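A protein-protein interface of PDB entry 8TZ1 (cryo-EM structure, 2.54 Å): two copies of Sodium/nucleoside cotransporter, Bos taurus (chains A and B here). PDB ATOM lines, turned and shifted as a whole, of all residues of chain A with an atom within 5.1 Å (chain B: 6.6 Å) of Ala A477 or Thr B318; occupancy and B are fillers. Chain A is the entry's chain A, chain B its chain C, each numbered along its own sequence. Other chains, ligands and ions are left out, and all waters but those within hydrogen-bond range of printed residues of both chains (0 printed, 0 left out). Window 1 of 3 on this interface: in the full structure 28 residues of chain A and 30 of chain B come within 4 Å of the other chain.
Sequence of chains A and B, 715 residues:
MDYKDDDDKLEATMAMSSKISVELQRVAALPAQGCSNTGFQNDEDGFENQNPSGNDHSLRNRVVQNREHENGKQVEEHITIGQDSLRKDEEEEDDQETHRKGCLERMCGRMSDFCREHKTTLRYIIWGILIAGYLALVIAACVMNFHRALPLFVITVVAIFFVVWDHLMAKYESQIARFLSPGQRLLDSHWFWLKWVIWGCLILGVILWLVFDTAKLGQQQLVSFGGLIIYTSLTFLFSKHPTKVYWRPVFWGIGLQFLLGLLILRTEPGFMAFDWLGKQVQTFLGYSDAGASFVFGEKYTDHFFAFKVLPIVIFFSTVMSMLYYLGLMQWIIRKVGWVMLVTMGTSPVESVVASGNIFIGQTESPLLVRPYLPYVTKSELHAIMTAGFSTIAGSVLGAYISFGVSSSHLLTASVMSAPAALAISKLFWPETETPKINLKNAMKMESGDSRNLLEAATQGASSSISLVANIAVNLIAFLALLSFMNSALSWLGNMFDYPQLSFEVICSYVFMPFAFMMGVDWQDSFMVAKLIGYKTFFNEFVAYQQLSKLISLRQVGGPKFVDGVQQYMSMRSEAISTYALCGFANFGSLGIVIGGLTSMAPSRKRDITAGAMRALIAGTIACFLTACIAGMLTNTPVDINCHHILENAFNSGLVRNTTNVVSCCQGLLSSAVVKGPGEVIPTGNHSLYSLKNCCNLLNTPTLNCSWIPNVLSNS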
ATOM      1  N   VAL A 473     -28.329  25.986  11.753  1.00  0.00           N
ATOM      2  CA  VAL A 473     -27.000  25.560  11.329  1.00  0.00           C
ATOM      3  C   VAL A 473     -26.965  25.338   9.821  1.00  0.00           C
ATOM      4  O   VAL A 473     -26.008  25.731   9.145  1.00  0.00           O
ATOM      5  CB  VAL A 473     -26.574  24.302  12.104  1.00  0.00           C
ATOM      6  CG1 VAL A 473     -25.179  23.867  11.715  1.00  0.00           C
ATOM      7  CG2 VAL A 473     -26.603  24.566  13.593  1.00  0.00           C
ATOM      8  N   ASN A 474     -27.999  24.699   9.270  1.00  0.00           N
ATOM      9  CA  ASN A 474     -28.028  24.456   7.831  1.00  0.00           C
ATOM     10  C   ASN A 474     -28.024  25.765   7.052  1.00  0.00           C
ATOM     11  O   ASN A 474     -27.354  25.877   6.020  1.00  0.00           O
ATOM     12  CB  ASN A 474     -29.250  23.615   7.464  1.00  0.00           C
ATOM     13  CG  ASN A 474     -29.024  22.135   7.680  1.00  0.00           C
ATOM     14  OD1 ASN A 474     -28.773  21.391   6.734  1.00  0.00           O
ATOM     15  ND2 ASN A 474     -29.104  21.698   8.928  1.00  0.00           N
ATOM     16  N   LEU A 475     -28.772  26.761   7.526  1.00  0.00           N
ATOM     17  CA  LEU A 475     -28.783  28.057   6.854  1.00  0.00           C
ATOM     18  C   LEU A 475     -27.407  28.707   6.888  1.00  0.00           C
ATOM     19  O   LEU A 475     -26.947  29.259   5.882  1.00  0.00           O
ATOM     20  CB  LEU A 475     -29.822  28.971   7.501  1.00  0.00           C
ATOM     21  CG  LEU A 475     -31.268  28.784   7.044  1.00  0.00           C
ATOM     22  CD1 LEU A 475     -32.188  29.593   7.922  1.00  0.00           C
ATOM     23  CD2 LEU A 475     -31.431  29.204   5.599  1.00  0.00           C
ATOM     24  N   ILE A 476     -26.734  28.655   8.038  1.00  0.00           N
ATOM     25  CA  ILE A 476     -25.403  29.245   8.145  1.00  0.00           C
ATOM     26  C   ILE A 476     -24.457  28.594   7.146  1.00  0.00           C
ATOM     27  O   ILE A 476     -23.728  29.275   6.417  1.00  0.00           O
ATOM     28  CB  ILE A 476     -24.876  29.116   9.584  1.00  0.00           C
ATOM     29  CG1 ILE A 476     -25.718  29.972  10.529  1.00  0.00           C
ATOM     30  CG2 ILE A 476     -23.417  29.532   9.650  1.00  0.00           C
ATOM     31  CD1 ILE A 476     -25.441  29.737  11.995  1.00  0.00           C
ATOM     32  N   ALA A 477     -24.450  27.261   7.105  1.00  0.00           N
ATOM     33  CA  ALA A 477     -23.543  26.556   6.210  1.00  0.00           C
ATOM     34  C   ALA A 477     -23.868  26.840   4.748  1.00  0.00           C
ATOM     35  O   ALA A 477     -22.966  27.098   3.944  1.00  0.00           O
ATOM     36  CB  ALA A 477     -23.605  25.057   6.487  1.00  0.00           C
ATOM     37  N   PHE A 478     -25.151  26.794   4.384  1.00  0.00           N
ATOM     38  CA  PHE A 478     -25.520  26.955   2.982  1.00  0.00           C
ATOM     39  C   PHE A 478     -25.187  28.349   2.469  1.00  0.00           C
ATOM     40  O   PHE A 478     -24.643  28.494   1.368  1.00  0.00           O
ATOM     41  CB  PHE A 478     -27.010  26.666   2.793  1.00  0.00           C
ATOM     42  CG  PHE A 478     -27.362  25.200   2.794  1.00  0.00           C
ATOM     43  CD1 PHE A 478     -26.460  24.240   2.364  1.00  0.00           C
ATOM     44  CD2 PHE A 478     -28.612  24.786   3.217  1.00  0.00           C
ATOM     45  CE1 PHE A 478     -26.796  22.907   2.365  1.00  0.00           C
ATOM     46  CE2 PHE A 478     -28.950  23.452   3.219  1.00  0.00           C
ATOM     47  CZ  PHE A 478     -28.041  22.512   2.792  1.00  0.00           C
ATOM     48  N   LEU A 479     -25.500  29.389   3.242  1.00  0.00           N
ATOM     49  CA  LEU A 479     -25.211  30.742   2.785  1.00  0.00           C
ATOM     50  C   LEU A 479     -23.711  30.995   2.730  1.00  0.00           C
ATOM     51  O   LEU A 479     -23.229  31.713   1.848  1.00  0.00           O
ATOM     52  CB  LEU A 479     -25.894  31.767   3.684  1.00  0.00           C
ATOM     53  CG  LEU A 479     -27.363  32.040   3.367  1.00  0.00           C
ATOM     54  CD1 LEU A 479     -28.246  30.997   3.991  1.00  0.00           C
ATOM     55  CD2 LEU A 479     -27.765  33.411   3.846  1.00  0.00           C
ATOM     56  N   ALA A 480     -22.958  30.423   3.670  1.00  0.00           N
ATOM     57  CA  ALA A 480     -21.505  30.531   3.609  1.00  0.00           C
ATOM     58  C   ALA A 480     -20.957  29.866   2.355  1.00  0.00           C
ATOM     59  O   ALA A 480     -20.069  30.412   1.690  1.00  0.00           O
ATOM     60  CB  ALA A 480     -20.884  29.915   4.858  1.00  0.00           C
ATOM     61  N   LEU A 481     -21.468  28.679   2.018  1.00  0.00           N
ATOM     62  CA  LEU A 481     -21.049  28.019   0.788  1.00  0.00           C
ATOM     63  C   LEU A 481     -21.438  28.837  -0.435  1.00  0.00           C
ATOM     64  O   LEU A 481     -20.671  28.929  -1.401  1.00  0.00           O
ATOM     65  CB  LEU A 481     -21.659  26.621   0.710  1.00  0.00           C
ATOM     66  CG  LEU A 481     -21.053  25.571   1.636  1.00  0.00           C
ATOM     67  CD1 LEU A 481     -21.962  24.365   1.700  1.00  0.00           C
ATOM     68  CD2 LEU A 481     -19.671  25.168   1.157  1.00  0.00           C
ATOM     69  N   LEU A 482     -22.631  29.435  -0.414  1.00  0.00           N
ATOM     70  CA  LEU A 482     -23.079  30.235  -1.547  1.00  0.00           C
ATOM     71  C   LEU A 482     -22.144  31.413  -1.790  1.00  0.00           C
ATOM     72  O   LEU A 482     -21.788  31.712  -2.935  1.00  0.00           O
ATOM     73  CB  LEU A 482     -24.507  30.718  -1.302  1.00  0.00           C
ATOM     74  CG  LEU A 482     -25.136  31.576  -2.397  1.00  0.00           C
ATOM     75  CD1 LEU A 482     -25.233  30.806  -3.696  1.00  0.00           C
ATOM     76  CD2 LEU A 482     -26.503  32.045  -1.958  1.00  0.00           C
ATOM     77  N   GLY B 291     -23.952  33.881   6.621  1.00  0.00           N
ATOM     78  CA  GLY B 291     -24.966  33.145   7.358  1.00  0.00           C
ATOM     79  C   GLY B 291     -25.223  33.722   8.736  1.00  0.00           C
ATOM     80  O   GLY B 291     -26.365  33.761   9.201  1.00  0.00           O
ATOM     81  N   VAL B 313     -16.757  27.783  13.190  1.00  0.00           N
ATOM     82  CA  VAL B 313     -16.602  26.364  13.494  1.00  0.00           C
ATOM     83  C   VAL B 313     -17.607  25.543  12.699  1.00  0.00           C
ATOM     84  O   VAL B 313     -17.281  24.474  12.169  1.00  0.00           O
ATOM     85  CB  VAL B 313     -16.749  26.126  15.009  1.00  0.00           C
ATOM     86  CG1 VAL B 313     -16.561  24.662  15.339  1.00  0.00           C
ATOM     87  CG2 VAL B 313     -15.752  26.971  15.776  1.00  0.00           C
ATOM     88  N   ILE B 314     -18.848  26.024  12.611  1.00  0.00           N
ATOM     89  CA  ILE B 314     -19.873  25.322  11.846  1.00  0.00           C
ATOM     90  C   ILE B 314     -19.466  25.222  10.382  1.00  0.00           C
ATOM     91  O   ILE B 314     -19.566  24.159   9.760  1.00  0.00           O
ATOM     92  CB  ILE B 314     -21.230  26.029  12.004  1.00  0.00           C
ATOM     93  CG1 ILE B 314     -21.730  25.895  13.441  1.00  0.00           C
ATOM     94  CG2 ILE B 314     -22.246  25.456  11.036  1.00  0.00           C
ATOM     95  CD1 ILE B 314     -22.876  26.812  13.780  1.00  0.00           C
ATOM     96  N   PHE B 315     -19.014  26.338   9.807  1.00  0.00           N
ATOM     97  CA  PHE B 315     -18.670  26.352   8.390  1.00  0.00           C
ATOM     98  C   PHE B 315     -17.502  25.423   8.091  1.00  0.00           C
ATOM     99  O   PHE B 315     -17.524  24.686   7.099  1.00  0.00           O
ATOM    100  CB  PHE B 315     -18.354  27.780   7.953  1.00  0.00           C
ATOM    101  CG  PHE B 315     -18.017  27.912   6.498  1.00  0.00           C
ATOM    102  CD1 PHE B 315     -18.777  27.272   5.536  1.00  0.00           C
ATOM    103  CD2 PHE B 315     -16.949  28.689   6.092  1.00  0.00           C
ATOM    104  CE1 PHE B 315     -18.468  27.396   4.201  1.00  0.00           C
ATOM    105  CE2 PHE B 315     -16.641  28.814   4.757  1.00  0.00           C
ATOM    106  CZ  PHE B 315     -17.400  28.169   3.813  1.00  0.00           C
ATOM    107  N   PHE B 316     -16.469  25.440   8.935  1.00  0.00           N
ATOM    108  CA  PHE B 316     -15.315  24.581   8.700  1.00  0.00           C
ATOM    109  C   PHE B 316     -15.679  23.109   8.835  1.00  0.00           C
ATOM    110  O   PHE B 316     -15.214  22.277   8.051  1.00  0.00           O
ATOM    111  CB  PHE B 316     -14.180  24.940   9.656  1.00  0.00           C
ATOM    112  CG  PHE B 316     -13.379  26.135   9.226  1.00  0.00           C
ATOM    113  CD1 PHE B 316     -13.954  27.143   8.475  1.00  0.00           C
ATOM    114  CD2 PHE B 316     -12.043  26.238   9.559  1.00  0.00           C
ATOM    115  CE1 PHE B 316     -13.211  28.234   8.079  1.00  0.00           C
ATOM    116  CE2 PHE B 316     -11.299  27.327   9.163  1.00  0.00           C
ATOM    117  CZ  PHE B 316     -11.884  28.324   8.422  1.00  0.00           C
ATOM    118  N   SER B 317     -16.509  22.767   9.822  1.00  0.00           N
ATOM    119  CA  SER B 317     -16.939  21.380   9.963  1.00  0.00           C
ATOM    120  C   SER B 317     -17.684  20.919   8.720  1.00  0.00           C
ATOM    121  O   SER B 317     -17.502  19.785   8.261  1.00  0.00           O
ATOM    122  CB  SER B 317     -17.822  21.226  11.199  1.00  0.00           C
ATOM    123  OG  SER B 317     -17.176  21.730  12.354  1.00  0.00           O
ATOM    124  N   THR B 318     -18.531  21.783   8.167  1.00  0.00           N
ATOM    125  CA  THR B 318     -19.233  21.451   6.935  1.00  0.00           C
ATOM    126  C   THR B 318     -18.252  21.177   5.801  1.00  0.00           C
ATOM    127  O   THR B 318     -18.373  20.176   5.087  1.00  0.00           O
ATOM    128  CB  THR B 318     -20.184  22.588   6.561  1.00  0.00           C
ATOM    129  OG1 THR B 318     -21.097  22.823   7.636  1.00  0.00           O
ATOM    130  CG2 THR B 318     -20.962  22.247   5.313  1.00  0.00           C
ATOM    131  N   VAL B 319     -17.262  22.054   5.631  1.00  0.00           N
ATOM    132  CA  VAL B 319     -16.305  21.893   4.541  1.00  0.00           C
ATOM    133  C   VAL B 319     -15.488  20.622   4.725  1.00  0.00           C
ATOM    134  O   VAL B 319     -15.197  19.911   3.756  1.00  0.00           O
ATOM    135  CB  VAL B 319     -15.405  23.136   4.439  1.00  0.00           C
ATOM    136  CG1 VAL B 319     -14.314  22.915   3.415  1.00  0.00           C
ATOM    137  CG2 VAL B 319     -16.229  24.347   4.072  1.00  0.00           C
ATOM    138  N   MET B 320     -15.102  20.314   5.963  1.00  0.00           N
ATOM    139  CA  MET B 320     -14.309  19.114   6.208  1.00  0.00           C
ATOM    140  C   MET B 320     -15.081  17.860   5.817  1.00  0.00           C
ATOM    141  O   MET B 320     -14.512  16.927   5.238  1.00  0.00           O
ATOM    142  CB  MET B 320     -13.894  19.056   7.676  1.00  0.00           C
ATOM    143  CG  MET B 320     -12.946  20.169   8.096  1.00  0.00           C
ATOM    144  SD  MET B 320     -11.271  19.949   7.483  1.00  0.00           S
ATOM    145  CE  MET B 320     -10.778  18.494   8.400  1.00  0.00           C
ATOM    146  N   SER B 321     -16.379  17.817   6.126  1.00  0.00           N
ATOM    147  CA  SER B 321     -17.196  16.676   5.730  1.00  0.00           C
ATOM    148  C   SER B 321     -17.281  16.562   4.214  1.00  0.00           C
ATOM    149  O   SER B 321     -17.229  15.457   3.662  1.00  0.00           O
ATOM    150  CB  SER B 321     -18.593  16.802   6.336  1.00  0.00           C
ATOM    151  OG  SER B 321     -19.305  17.880   5.760  1.00  0.00           O
ATOM    152  N   MET B 322     -17.424  17.693   3.524  1.00  0.00           N
ATOM    153  CA  MET B 322     -17.483  17.677   2.067  1.00  0.00           C
ATOM    154  C   MET B 322     -16.183  17.149   1.475  1.00  0.00           C
ATOM    155  O   MET B 322     -16.194  16.357   0.527  1.00  0.00           O
ATOM    156  CB  MET B 322     -17.780  19.084   1.547  1.00  0.00           C
ATOM    157  CG  MET B 322     -19.090  19.670   2.054  1.00  0.00           C
ATOM    158  SD  MET B 322     -19.259  21.434   1.739  1.00  0.00           S
ATOM    159  CE  MET B 322     -19.639  21.421  -0.007  1.00  0.00           C
ATOM    160  N   LEU B 323     -15.045  17.584   2.021  1.00  0.00           N
ATOM    161  CA  LEU B 323     -13.758  17.092   1.542  1.00  0.00           C
ATOM    162  C   LEU B 323     -13.608  15.599   1.802  1.00  0.00           C
ATOM    163  O   LEU B 323     -13.075  14.866   0.962  1.00  0.00           O
ATOM    164  CB  LEU B 323     -12.622  17.866   2.204  1.00  0.00           C
ATOM    165  CG  LEU B 323     -12.510  19.350   1.857  1.00  0.00           C
ATOM    166  CD1 LEU B 323     -11.442  20.009   2.702  1.00  0.00           C
ATOM    167  CD2 LEU B 323     -12.196  19.528   0.388  1.00  0.00           C
ATOM    168  N   ALA B 456     -23.621  15.382   2.503  1.00  0.00           N
ATOM    169  CA  ALA B 456     -22.430  15.457   3.339  1.00  0.00           C
ATOM    170  C   ALA B 456     -22.357  16.789   4.071  1.00  0.00           C
ATOM    171  O   ALA B 456     -21.983  16.842   5.248  1.00  0.00           O
ATOM    172  CB  ALA B 456     -21.184  15.247   2.482  1.00  0.00           C
ATOM    173  N   ALA B 457     -22.702  17.879   3.384  1.00  0.00           N
ATOM    174  CA  ALA B 457     -22.699  19.189   4.026  1.00  0.00           C
ATOM    175  C   ALA B 457     -23.686  19.243   5.183  1.00  0.00           C
ATOM    176  O   ALA B 457     -23.372  19.782   6.251  1.00  0.00           O
ATOM    177  CB  ALA B 457     -23.021  20.269   2.995  1.00  0.00           C
ATOM    178  N   THR B 458     -24.891  18.699   4.991  1.00  0.00           N
ATOM    179  CA  THR B 458     -25.876  18.690   6.067  1.00  0.00           C
ATOM    180  C   THR B 458     -25.388  17.866   7.251  1.00  0.00           C
ATOM    181  O   THR B 458     -25.554  18.268   8.407  1.00  0.00           O
ATOM    182  CB  THR B 458     -27.209  18.144   5.558  1.00  0.00           C
ATOM    183  OG1 THR B 458     -27.033  16.799   5.096  1.00  0.00           O
ATOM    184  CG2 THR B 458     -27.744  19.002   4.426  1.00  0.00           C
ATOM    185  N   GLN B 459     -24.787  16.705   6.982  1.00  0.00           N
ATOM    186  CA  GLN B 459     -24.278  15.874   8.066  1.00  0.00           C
ATOM    187  C   GLN B 459     -23.183  16.593   8.841  1.00  0.00           C
ATOM    188  O   GLN B 459     -23.148  16.538  10.077  1.00  0.00           O
ATOM    189  CB  GLN B 459     -23.759  14.550   7.508  1.00  0.00           C
ATOM    190  CG  GLN B 459     -24.856  13.578   7.117  1.00  0.00           C
ATOM    191  CD  GLN B 459     -24.318  12.322   6.464  1.00  0.00           C
ATOM    192  OE1 GLN B 459     -23.107  12.112   6.401  1.00  0.00           O
ATOM    193  NE2 GLN B 459     -25.217  11.481   5.970  1.00  0.00           N
ATOM    194  N   GLY B 460     -22.277  17.268   8.136  1.00  0.00           N
ATOM    195  CA  GLY B 460     -21.248  18.031   8.819  1.00  0.00           C
ATOM    196  C   GLY B 460     -21.823  19.158   9.652  1.00  0.00           C
ATOM    197  O   GLY B 460     -21.348  19.432  10.757  1.00  0.00           O
ATOM    198  N   ALA B 461     -22.848  19.831   9.132  1.00  0.00           N
ATOM    199  CA  ALA B 461     -23.494  20.899   9.886  1.00  0.00           C
ATOM    200  C   ALA B 461     -24.126  20.364  11.165  1.00  0.00           C
ATOM    201  O   ALA B 461     -23.942  20.935  12.246  1.00  0.00           O
ATOM    202  CB  ALA B 461     -24.543  21.585   9.013  1.00  0.00           C
ATOM    203  N   SER B 462     -24.866  19.260  11.065  1.00  0.00           N
ATOM    204  CA  SER B 462     -25.553  18.724  12.234  1.00  0.00           C
ATOM    205  C   SER B 462     -24.566  18.343  13.331  1.00  0.00           C
ATOM    206  O   SER B 462     -24.826  18.571  14.519  1.00  0.00           O
ATOM    207  CB  SER B 462     -26.397  17.516  11.836  1.00  0.00           C
ATOM    208  OG  SER B 462     -25.577  16.436  11.426  1.00  0.00           O
ATOM    209  N   SER B 464     -21.865  19.703  14.136  1.00  0.00           N
ATOM    210  CA  SER B 464     -21.278  20.868  14.788  1.00  0.00           C
ATOM    211  C   SER B 464     -22.127  21.405  15.932  1.00  0.00           C
ATOM    212  O   SER B 464     -21.646  22.258  16.684  1.00  0.00           O
ATOM    213  CB  SER B 464     -21.052  21.978  13.761  1.00  0.00           C
ATOM    214  OG  SER B 464     -22.282  22.450  13.243  1.00  0.00           O
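Of the 10 printed residues of chain A, 6 touch a printed residue of chain B.
Of the 20 printed residues of chain B, 7 touch a printed residue of chain A.
Printed residues of chain B that touch a printed residue of chain A: Ile B314, Phe B315, Thr B318, Met B322, Thr B458, Ala B461 and Ser B464.
Among the printed residues, no Asp or Glu carboxylate lies within 4 Å of a Lys or Arg side-chain nitrogen of the other chain.
Thr B318 touches just one residue of chain A: Ala A477.
Printed residues of chain A within 4 Å of Ala B461: Val A473 (3.2 Å).
Printed residues of chain B within 4 Å of Val A473: Ile B314 (3.4 Å), Ala B461 (3.2 Å) and Ser B464 (3.6 Å).
Gln B459 touches none of the printed residues of chain A.
Gly B460 touches none of the printed residues of chain A.
The nearest residue of chain B that does not touch Ala A477 is Ala B461 (4.4 Å).
The nearest residue of chain A that does not touch Thr B318 is Leu A481 (4.3 Å).
The nearest printed residue of chain A that does not touch Ile B314 is Ile A476 (4.3 Å).
O of Ile B314 sits at hydrogen-bond distance from OG1 of Thr B318 (2.9 Å).
The backbone carbonyl oxygen of Thr B318 is in hydrogen-bond range of the side-chain hydroxyl of Ser B321 (2.6 Å).
The side-chain hydroxyl of Ser B464 lies within hydrogen-bond range of the backbone carbonyl oxygen of Ala B461.
No position is printed for both chains.
Of the 9 pairs that touch across the chains among the printed residues, none has its exchanged pair printed and touching as well.
CG2 of Ile B314 touches CG1 of Val A473, at 3.4 Å.
Ala B461 touches Val A473 (O to CG1, 3.2 Å).
Ser B464 touches Val A473 (OG to CG1, 3.6 Å).
Thr B458 touches Asn A474 (CG2 to OD1, 3.5 Å).
Ala A477 touches Thr B318.
CG2 of Thr B458 touches CZ of Phe A478, 3.9 Å away.
CB of Ala A480 touches CD1 of Phe B315 (3.4 Å).
Leu A481 touches Phe B315 (N to CE1, 3.9 Å).
CD2 of Leu A481 touches SD of Met B322 (3.8 Å).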
